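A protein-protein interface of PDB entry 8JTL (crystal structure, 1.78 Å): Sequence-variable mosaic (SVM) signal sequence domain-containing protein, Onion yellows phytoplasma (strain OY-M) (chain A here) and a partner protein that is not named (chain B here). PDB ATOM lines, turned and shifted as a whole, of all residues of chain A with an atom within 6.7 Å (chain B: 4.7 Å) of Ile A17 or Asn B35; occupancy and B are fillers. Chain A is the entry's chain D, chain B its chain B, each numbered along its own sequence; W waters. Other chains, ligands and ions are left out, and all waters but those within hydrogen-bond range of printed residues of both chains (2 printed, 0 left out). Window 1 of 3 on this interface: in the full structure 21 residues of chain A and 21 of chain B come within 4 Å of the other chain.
Printed residues of chain B within 4 Å of Val A15: Leu B74 (3.5 Å).
Asn A16 touches none of the printed residues of chain B.
Ile A17 touches two residues of chain B.
Printed residues of chain B within 4 Å of Gln A29: Gly B39 (2.9 Å).
Of the printed residues of chain B, Tyr A97 touches Leu B74.
Asn B35 touches just these residues of chain A: Ile A17 and Phe A28.
The nearest printed residue of chain B that does not touch Ile A17 is Thr B31 (6.3 Å).
The nearest printed residue of chain B that does not touch Phe A31 is Gly B39 (5.7 Å).
Of the 15 printed residues of chain A, 8 touch a printed residue of chain B.
Hydrophobic or aromatic side chains of chain A that line the printed part of chain B: Val A15, Ile A17, Phe A19, Phe A28, Phe A31 and Tyr A97.
Hydrophobic or aromatic side chains of chain B within 4 Å of the printed part of chain A: Leu B36 and Leu B74.
Along chain B the printed residues that touch a printed residue of chain A span positions 32 to 74.
Among the printed residues, 11 pairs touch across the chains.
Water W2 bridges O of Thr A18 (2.6 Å) and ND2 of Asn B35 (2.7 Å).
Water W1 lies within hydrogen-bond range of the backbone carbonyl oxygen of Leu B36 (2.6 Å) and the backbone NH of Gln A29 (2.8 Å).
Val A15 touches Leu B74.
CG2 of Ile A17 touches ND2 of Asn B35 (3.6 Å).
Leu B74 touches Ile A17.
Thr A18 touches Glu B32.
Glu B32 touches Phe A19.
Asn B35 touches Phe A28.
CB of Phe A28 touches CD2 of Leu B36, at 3.3 Å.
Phe A28 touches Leu B74.
CD1 of Leu B74 touches CE2 of Phe A31 (3.5 Å).
Tyr A97 touches Leu B74 (CE1 to CD1, 3.7 Å).
The backbone carbonyl oxygen (O) of Val A15 lies within hydrogen-bond range of the backbone NH (N) of Ile A98, at 2.8 Å.
The backbone carbonyl oxygen (O) of Ile A17 is in hydrogen-bond range of the backbone NH (N) of Trp A100 (2.7 Å).
N of Phe A19 is in hydrogen-bond range of O of Trp A100.
The side-chain amide nitrogen (ND2) of Asn B35 is in hydrogen-bond range of the backbone carbonyl oxygen (O) of Thr B31 (3.1 Å).
The backbone NH (N) of Ile A17 is in hydrogen-bond range of the backbone carbonyl oxygen (O) of Ile A98 (2.8 Å).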
ATOM      1  N   VAL A  15      -3.793   1.985  25.181  1.00  0.00           N
ATOM      2  CA  VAL A  15      -5.229   2.109  25.179  1.00  0.00           C
ATOM      3  C   VAL A  15      -5.716   1.246  26.305  1.00  0.00           C
ATOM      4  O   VAL A  15      -5.655   0.008  26.230  1.00  0.00           O
ATOM      5  CB  VAL A  15      -5.843   1.674  23.849  1.00  0.00           C
ATOM      6  CG1 VAL A  15      -7.329   1.952  23.844  1.00  0.00           C
ATOM      7  CG2 VAL A  15      -5.151   2.402  22.700  1.00  0.00           C
ATOM      8  N   ASN A  16      -6.157   1.890  27.361  1.00  0.00           N
ATOM      9  CA  ASN A  16      -6.638   1.190  28.527  1.00  0.00           C
ATOM     10  C   ASN A  16      -8.124   0.986  28.345  1.00  0.00           C
ATOM     11  O   ASN A  16      -8.863   1.921  28.061  1.00  0.00           O
ATOM     12  CB  ASN A  16      -6.353   2.000  29.779  1.00  0.00           C
ATOM     13  CG  ASN A  16      -4.889   2.129  30.014  1.00  0.00           C
ATOM     14  OD1 ASN A  16      -4.276   1.224  30.522  1.00  0.00           O
ATOM     15  ND2 ASN A  16      -4.306   3.250  29.573  1.00  0.00           N
ATOM     16  N   ILE A  17      -8.543  -0.242  28.465  1.00  0.00           N
ATOM     17  CA  ILE A  17      -9.934  -0.595  28.264  1.00  0.00           C
ATOM     18  C   ILE A  17     -10.345  -1.410  29.449  1.00  0.00           C
ATOM     19  O   ILE A  17      -9.660  -2.364  29.803  1.00  0.00           O
ATOM     20  CB  ILE A  17     -10.116  -1.426  26.990  1.00  0.00           C
ATOM     21  CG1 ILE A  17      -9.392  -0.761  25.821  1.00  0.00           C
ATOM     22  CG2 ILE A  17     -11.576  -1.627  26.758  1.00  0.00           C
ATOM     23  CD1 ILE A  17      -9.540  -1.575  24.529  1.00  0.00           C
ATOM     24  N   THR A  18     -11.456  -1.058  30.053  1.00  0.00           N
ATOM     25  CA  THR A  18     -11.869  -1.732  31.259  1.00  0.00           C
ATOM     26  C   THR A  18     -13.192  -2.431  31.054  1.00  0.00           C
ATOM     27  O   THR A  18     -14.108  -1.865  30.471  1.00  0.00           O
ATOM     28  CB  THR A  18     -11.970  -0.744  32.391  1.00  0.00           C
ATOM     29  OG1 THR A  18     -10.660  -0.204  32.602  1.00  0.00           O
ATOM     30  CG2 THR A  18     -12.384  -1.432  33.637  1.00  0.00           C
ATOM     31  N   PHE A  19     -13.255  -3.665  31.518  1.00  0.00           N
ATOM     32  CA  PHE A  19     -14.462  -4.467  31.443  1.00  0.00           C
ATOM     33  C   PHE A  19     -14.783  -4.964  32.832  1.00  0.00           C
ATOM     34  O   PHE A  19     -13.880  -5.318  33.596  1.00  0.00           O
ATOM     35  CB  PHE A  19     -14.269  -5.643  30.498  1.00  0.00           C
ATOM     36  CG  PHE A  19     -14.372  -5.242  29.058  1.00  0.00           C
ATOM     37  CD1 PHE A  19     -15.597  -5.159  28.452  1.00  0.00           C
ATOM     38  CD2 PHE A  19     -13.242  -4.910  28.342  1.00  0.00           C
ATOM     39  CE1 PHE A  19     -15.723  -4.769  27.109  1.00  0.00           C
ATOM     40  CE2 PHE A  19     -13.356  -4.503  27.021  1.00  0.00           C
ATOM     41  CZ  PHE A  19     -14.589  -4.445  26.395  1.00  0.00           C
ATOM     42  N   ILE A  25     -15.222  -9.467  26.421  1.00  0.00           N
ATOM     43  CA  ILE A  25     -14.282  -9.238  25.348  1.00  0.00           C
ATOM     44  C   ILE A  25     -14.478 -10.253  24.259  1.00  0.00           C
ATOM     45  O   ILE A  25     -14.066 -10.028  23.121  1.00  0.00           O
ATOM     46  CB  ILE A  25     -12.861  -9.260  25.894  1.00  0.00           C
ATOM     47  CG1 ILE A  25     -12.695  -8.076  26.857  1.00  0.00           C
ATOM     48  CG2 ILE A  25     -11.814  -9.274  24.748  1.00  0.00           C
ATOM     49  CD1 ILE A  25     -11.418  -8.146  27.672  1.00  0.00           C
ATOM     50  N   PHE A  28     -15.835  -8.402  21.558  1.00  0.00           N
ATOM     51  CA  PHE A  28     -15.072  -7.211  21.251  1.00  0.00           C
ATOM     52  C   PHE A  28     -14.170  -7.483  20.065  1.00  0.00           C
ATOM     53  O   PHE A  28     -13.056  -7.972  20.210  1.00  0.00           O
ATOM     54  CB  PHE A  28     -14.287  -6.810  22.491  1.00  0.00           C
ATOM     55  CG  PHE A  28     -13.741  -5.440  22.446  1.00  0.00           C
ATOM     56  CD1 PHE A  28     -14.011  -4.590  21.393  1.00  0.00           C
ATOM     57  CD2 PHE A  28     -12.933  -4.997  23.475  1.00  0.00           C
ATOM     58  CE1 PHE A  28     -13.507  -3.309  21.367  1.00  0.00           C
ATOM     59  CE2 PHE A  28     -12.417  -3.707  23.468  1.00  0.00           C
ATOM     60  CZ  PHE A  28     -12.710  -2.856  22.410  1.00  0.00           C
ATOM     61  N   GLN A  29     -14.637  -7.129  18.918  1.00  0.00           N
ATOM     62  CA  GLN A  29     -13.795  -7.181  17.744  1.00  0.00           C
ATOM     63  C   GLN A  29     -12.840  -6.011  17.759  1.00  0.00           C
ATOM     64  O   GLN A  29     -13.220  -4.920  18.173  1.00  0.00           O
ATOM     65  CB  GLN A  29     -14.649  -7.102  16.489  1.00  0.00           C
ATOM     66  CG  GLN A  29     -15.671  -8.170  16.421  1.00  0.00           C
ATOM     67  CD  GLN A  29     -16.423  -8.060  15.130  1.00  0.00           C
ATOM     68  OE1 GLN A  29     -17.623  -7.832  15.128  1.00  0.00           O
ATOM     69  NE2 GLN A  29     -15.700  -8.145  14.013  1.00  0.00           N
ATOM     70  N   PHE A  31     -10.415  -7.687  19.063  1.00  0.00           N
ATOM     71  CA  PHE A  31      -9.563  -8.211  20.119  1.00  0.00           C
ATOM     72  C   PHE A  31      -9.903  -9.625  20.492  1.00  0.00           C
ATOM     73  O   PHE A  31      -9.001 -10.381  20.865  1.00  0.00           O
ATOM     74  CB  PHE A  31      -9.668  -7.306  21.334  1.00  0.00           C
ATOM     75  CG  PHE A  31      -9.360  -5.929  20.990  1.00  0.00           C
ATOM     76  CD1 PHE A  31      -8.071  -5.620  20.564  1.00  0.00           C
ATOM     77  CD2 PHE A  31     -10.321  -4.976  20.977  1.00  0.00           C
ATOM     78  CE1 PHE A  31      -7.765  -4.342  20.168  1.00  0.00           C
ATOM     79  CE2 PHE A  31     -10.012  -3.682  20.581  1.00  0.00           C
ATOM     80  CZ  PHE A  31      -8.742  -3.370  20.194  1.00  0.00           C
ATOM     81  N   LEU A  65      -6.330  -7.686  32.873  1.00  0.00           N
ATOM     82  CA  LEU A  65      -6.922  -8.801  32.149  1.00  0.00           C
ATOM     83  C   LEU A  65      -6.036  -9.287  31.018  1.00  0.00           C
ATOM     84  O   LEU A  65      -6.010 -10.472  30.714  1.00  0.00           O
ATOM     85  CB  LEU A  65      -8.284  -8.395  31.574  1.00  0.00           C
ATOM     86  CG  LEU A  65      -9.282  -8.183  32.685  1.00  0.00           C
ATOM     87  CD1 LEU A  65     -10.584  -7.869  32.020  1.00  0.00           C
ATOM     88  CD2 LEU A  65      -9.429  -9.428  33.567  1.00  0.00           C
ATOM     89  N   TYR A  97      -3.042  -2.353  23.727  1.00  0.00           N
ATOM     90  CA  TYR A  97      -4.314  -2.416  24.409  1.00  0.00           C
ATOM     91  C   TYR A  97      -4.112  -3.117  25.722  1.00  0.00           C
ATOM     92  O   TYR A  97      -3.660  -4.263  25.762  1.00  0.00           O
ATOM     93  CB  TYR A  97      -5.338  -3.169  23.577  1.00  0.00           C
ATOM     94  CG  TYR A  97      -5.626  -2.422  22.331  1.00  0.00           C
ATOM     95  CD1 TYR A  97      -6.605  -1.442  22.302  1.00  0.00           C
ATOM     96  CD2 TYR A  97      -4.890  -2.657  21.185  1.00  0.00           C
ATOM     97  CE1 TYR A  97      -6.895  -0.748  21.121  1.00  0.00           C
ATOM     98  CE2 TYR A  97      -5.184  -2.005  20.020  1.00  0.00           C
ATOM     99  CZ  TYR A  97      -6.171  -1.050  19.983  1.00  0.00           C
ATOM    100  OH  TYR A  97      -6.386  -0.416  18.784  1.00  0.00           O
ATOM    101  N   ILE A  98      -4.431  -2.426  26.790  1.00  0.00           N
ATOM    102  CA  ILE A  98      -4.342  -2.992  28.108  1.00  0.00           C
ATOM    103  C   ILE A  98      -5.745  -3.143  28.624  1.00  0.00           C
ATOM    104  O   ILE A  98      -6.474  -2.162  28.772  1.00  0.00           O
ATOM    105  CB  ILE A  98      -3.504  -2.125  29.031  1.00  0.00           C
ATOM    106  CG1 ILE A  98      -2.158  -1.862  28.333  1.00  0.00           C
ATOM    107  CG2 ILE A  98      -3.374  -2.843  30.326  1.00  0.00           C
ATOM    108  CD1 ILE A  98      -1.287  -1.001  29.182  1.00  0.00           C
ATOM    109  N   PHE A  99      -6.145  -4.380  28.829  1.00  0.00           N
ATOM    110  CA  PHE A  99      -7.488  -4.667  29.265  1.00  0.00           C
ATOM    111  C   PHE A  99      -7.473  -4.833  30.752  1.00  0.00           C
ATOM    112  O   PHE A  99      -6.625  -5.532  31.307  1.00  0.00           O
ATOM    113  CB  PHE A  99      -8.044  -5.908  28.619  1.00  0.00           C
ATOM    114  CG  PHE A  99      -8.053  -5.823  27.157  1.00  0.00           C
ATOM    115  CD1 PHE A  99      -6.915  -6.085  26.442  1.00  0.00           C
ATOM    116  CD2 PHE A  99      -9.215  -5.449  26.485  1.00  0.00           C
ATOM    117  CE1 PHE A  99      -6.927  -6.038  25.063  1.00  0.00           C
ATOM    118  CE2 PHE A  99      -9.217  -5.362  25.101  1.00  0.00           C
ATOM    119  CZ  PHE A  99      -8.066  -5.658  24.392  1.00  0.00           C
ATOM    120  N   TRP A 100      -8.425  -4.209  31.375  1.00  0.00           N
ATOM    121  CA  TRP A 100      -8.470  -4.106  32.810  1.00  0.00           C
ATOM    122  C   TRP A 100      -9.815  -4.595  33.271  1.00  0.00           C
ATOM    123  O   TRP A 100     -10.820  -4.396  32.590  1.00  0.00           O
ATOM    124  CB  TRP A 100      -8.328  -2.683  33.269  1.00  0.00           C
ATOM    125  CG  TRP A 100      -7.068  -2.056  32.928  1.00  0.00           C
ATOM    126  CD1 TRP A 100      -6.842  -1.202  31.890  1.00  0.00           C
ATOM    127  CD2 TRP A 100      -5.827  -2.199  33.623  1.00  0.00           C
ATOM    128  NE1 TRP A 100      -5.529  -0.769  31.944  1.00  0.00           N
ATOM    129  CE2 TRP A 100      -4.900  -1.363  32.996  1.00  0.00           C
ATOM    130  CE3 TRP A 100      -5.422  -2.927  34.743  1.00  0.00           C
ATOM    131  CZ2 TRP A 100      -3.576  -1.240  33.443  1.00  0.00           C
ATOM    132  CZ3 TRP A 100      -4.112  -2.813  35.180  1.00  0.00           C
ATOM    133  CH2 TRP A 100      -3.204  -1.986  34.529  1.00  0.00           C
ATOM    134  N   GLN A 101      -9.840  -5.125  34.455  1.00  0.00           N
ATOM    135  CA  GLN A 101     -11.057  -5.542  35.060  1.00  0.00           C
ATOM    136  C   GLN A 101     -11.572  -4.452  35.965  1.00  0.00           C
ATOM    137  O   GLN A 101     -10.843  -3.925  36.785  1.00  0.00           O
ATOM    138  CB  GLN A 101     -10.810  -6.753  35.915  1.00  0.00           C
ATOM    139  CG  GLN A 101     -11.938  -7.128  36.831  1.00  0.00           C
ATOM    140  CD  GLN A 101     -12.312  -8.567  36.682  1.00  0.00           C
ATOM    141  OE1 GLN A 101     -11.598  -9.452  37.132  1.00  0.00           O
ATOM    142  NE2 GLN A 101     -13.432  -8.810  36.051  1.00  0.00           N
ATOM    143  N   THR B  31     -19.730   2.529  28.513  1.00  0.00           N
ATOM    144  CA  THR B  31     -18.395   2.504  27.937  1.00  0.00           C
ATOM    145  C   THR B  31     -18.111   1.159  27.302  1.00  0.00           C
ATOM    146  O   THR B  31     -17.531   1.080  26.221  1.00  0.00           O
ATOM    147  CB  THR B  31     -17.356   2.801  29.023  1.00  0.00           C
ATOM    148  OG1 THR B  31     -17.516   4.153  29.443  1.00  0.00           O
ATOM    149  CG2 THR B  31     -15.970   2.564  28.484  1.00  0.00           C
ATOM    150  N   GLU B  32     -18.527   0.088  27.949  1.00  0.00           N
ATOM    151  CA  GLU B  32     -18.249  -1.220  27.379  1.00  0.00           C
ATOM    152  C   GLU B  32     -19.051  -1.414  26.115  1.00  0.00           C
ATOM    153  O   GLU B  32     -18.522  -1.902  25.106  1.00  0.00           O
ATOM    154  CB  GLU B  32     -18.571  -2.314  28.370  1.00  0.00           C
ATOM    155  CG  GLU B  32     -17.741  -2.209  29.590  1.00  0.00           C
ATOM    156  CD  GLU B  32     -17.914  -3.404  30.478  1.00  0.00           C
ATOM    157  OE1 GLU B  32     -18.434  -4.437  30.007  1.00  0.00           O
ATOM    158  OE2 GLU B  32     -17.494  -3.325  31.648  1.00  0.00           O
ATOM    159  N   ALA B  33     -20.330  -1.037  26.158  1.00  0.00           N
ATOM    160  CA  ALA B  33     -21.128  -1.119  24.934  1.00  0.00           C
ATOM    161  C   ALA B  33     -20.487  -0.292  23.847  1.00  0.00           C
ATOM    162  O   ALA B  33     -20.412  -0.710  22.680  1.00  0.00           O
ATOM    163  CB  ALA B  33     -22.563  -0.654  25.193  1.00  0.00           C
ATOM    164  N   VAL B  34     -20.039   0.908  24.202  1.00  0.00           N
ATOM    165  CA  VAL B  34     -19.435   1.764  23.204  1.00  0.00           C
ATOM    166  C   VAL B  34     -18.177   1.123  22.650  1.00  0.00           C
ATOM    167  O   VAL B  34     -17.964   1.088  21.436  1.00  0.00           O
ATOM    168  CB  VAL B  34     -19.161   3.161  23.774  1.00  0.00           C
ATOM    169  CG1 VAL B  34     -18.374   3.939  22.767  1.00  0.00           C
ATOM    170  CG2 VAL B  34     -20.484   3.851  24.069  1.00  0.00           C
ATOM    171  N   ASN B  35     -17.311   0.626  23.527  1.00  0.00           N
ATOM    172  CA  ASN B  35     -16.095   0.021  23.030  1.00  0.00           C
ATOM    173  C   ASN B  35     -16.412  -1.107  22.091  1.00  0.00           C
ATOM    174  O   ASN B  35     -15.813  -1.210  21.026  1.00  0.00           O
ATOM    175  CB  ASN B  35     -15.235  -0.478  24.176  1.00  0.00           C
ATOM    176  CG  ASN B  35     -14.661   0.666  24.938  1.00  0.00           C
ATOM    177  OD1 ASN B  35     -14.554   1.752  24.396  1.00  0.00           O
ATOM    178  ND2 ASN B  35     -14.442   0.486  26.207  1.00  0.00           N
ATOM    179  N   LEU B  36     -17.324  -1.977  22.493  1.00  0.00           N
ATOM    180  CA  LEU B  36     -17.672  -3.102  21.643  1.00  0.00           C
ATOM    181  C   LEU B  36     -18.179  -2.615  20.310  1.00  0.00           C
ATOM    182  O   LEU B  36     -17.895  -3.212  19.270  1.00  0.00           O
ATOM    183  CB  LEU B  36     -18.753  -3.961  22.309  1.00  0.00           C
ATOM    184  CG  LEU B  36     -18.410  -4.783  23.539  1.00  0.00           C
ATOM    185  CD1 LEU B  36     -19.557  -5.691  23.862  1.00  0.00           C
ATOM    186  CD2 LEU B  36     -17.295  -5.586  23.159  1.00  0.00           C
ATOM    187  N   LEU B  37     -18.977  -1.552  20.338  1.00  0.00           N
ATOM    188  CA  LEU B  37     -19.558  -1.002  19.126  1.00  0.00           C
ATOM    189  C   LEU B  37     -18.476  -0.413  18.247  1.00  0.00           C
ATOM    190  O   LEU B  37     -18.501  -0.601  17.028  1.00  0.00           O
ATOM    191  CB  LEU B  37     -20.589   0.045  19.507  1.00  0.00           C
ATOM    192  CG  LEU B  37     -21.543   0.567  18.460  1.00  0.00           C
ATOM    193  CD1 LEU B  37     -22.217  -0.648  17.831  1.00  0.00           C
ATOM    194  CD2 LEU B  37     -22.489   1.449  19.240  1.00  0.00           C
ATOM    195  N   CYS B  38     -17.514   0.314  18.849  1.00  0.00           N
ATOM    196  CA  CYS B  38     -16.392   0.805  18.055  1.00  0.00           C
ATOM    197  C   CYS B  38     -15.647  -0.335  17.417  1.00  0.00           C
ATOM    198  O   CYS B  38     -15.241  -0.249  16.249  1.00  0.00           O
ATOM    199  CB  CYS B  38     -15.422   1.629  18.907  1.00  0.00           C
ATOM    200  SG  CYS B  38     -16.211   3.051  19.573  1.00  0.00           S
ATOM    201  N   GLY B  39     -15.421  -1.400  18.188  1.00  0.00           N
ATOM    202  CA  GLY B  39     -14.791  -2.572  17.620  1.00  0.00           C
ATOM    203  C   GLY B  39     -15.622  -3.151  16.489  1.00  0.00           C
ATOM    204  O   GLY B  39     -15.130  -3.374  15.381  1.00  0.00           O
ATOM    205  N   LEU B  74     -10.787   4.100  20.859  1.00  0.00           N
ATOM    206  CA  LEU B  74     -10.889   3.471  22.156  1.00  0.00           C
ATOM    207  C   LEU B  74     -10.148   4.276  23.207  1.00  0.00           C
ATOM    208  O   LEU B  74     -10.595   4.352  24.353  1.00  0.00           O
ATOM    209  CB  LEU B  74     -10.329   2.064  22.062  1.00  0.00           C
ATOM    210  CG  LEU B  74     -11.185   1.151  21.201  1.00  0.00           C
ATOM    211  CD1 LEU B  74     -10.557  -0.270  21.193  1.00  0.00           C
ATOM    212  CD2 LEU B  74     -12.591   1.138  21.771  1.00  0.00           C
ATOM    213  N   MET B  77     -12.176   6.585  25.212  1.00  0.00           N
ATOM    214  CA  MET B  77     -13.145   6.101  26.170  1.00  0.00           C
ATOM    215  C   MET B  77     -12.565   6.079  27.574  1.00  0.00           C
ATOM    216  O   MET B  77     -13.302   5.827  28.540  1.00  0.00           O
ATOM    217  CB  MET B  77     -13.591   4.701  25.738  1.00  0.00           C
ATOM    218  CG  MET B  77     -14.663   4.717  24.617  1.00  0.00           C
ATOM    219  SD  MET B  77     -15.726   6.143  24.617  1.00  0.00           S
ATOM    220  CE  MET B  77     -16.898   5.512  25.820  1.00  0.00           C
HETATM  221  O   HOH W   1     -17.001  -5.642  19.063  1.00  0.00           O
HETATM  222  O   HOH W   2     -14.695  -1.546  27.963  1.00  0.00           O
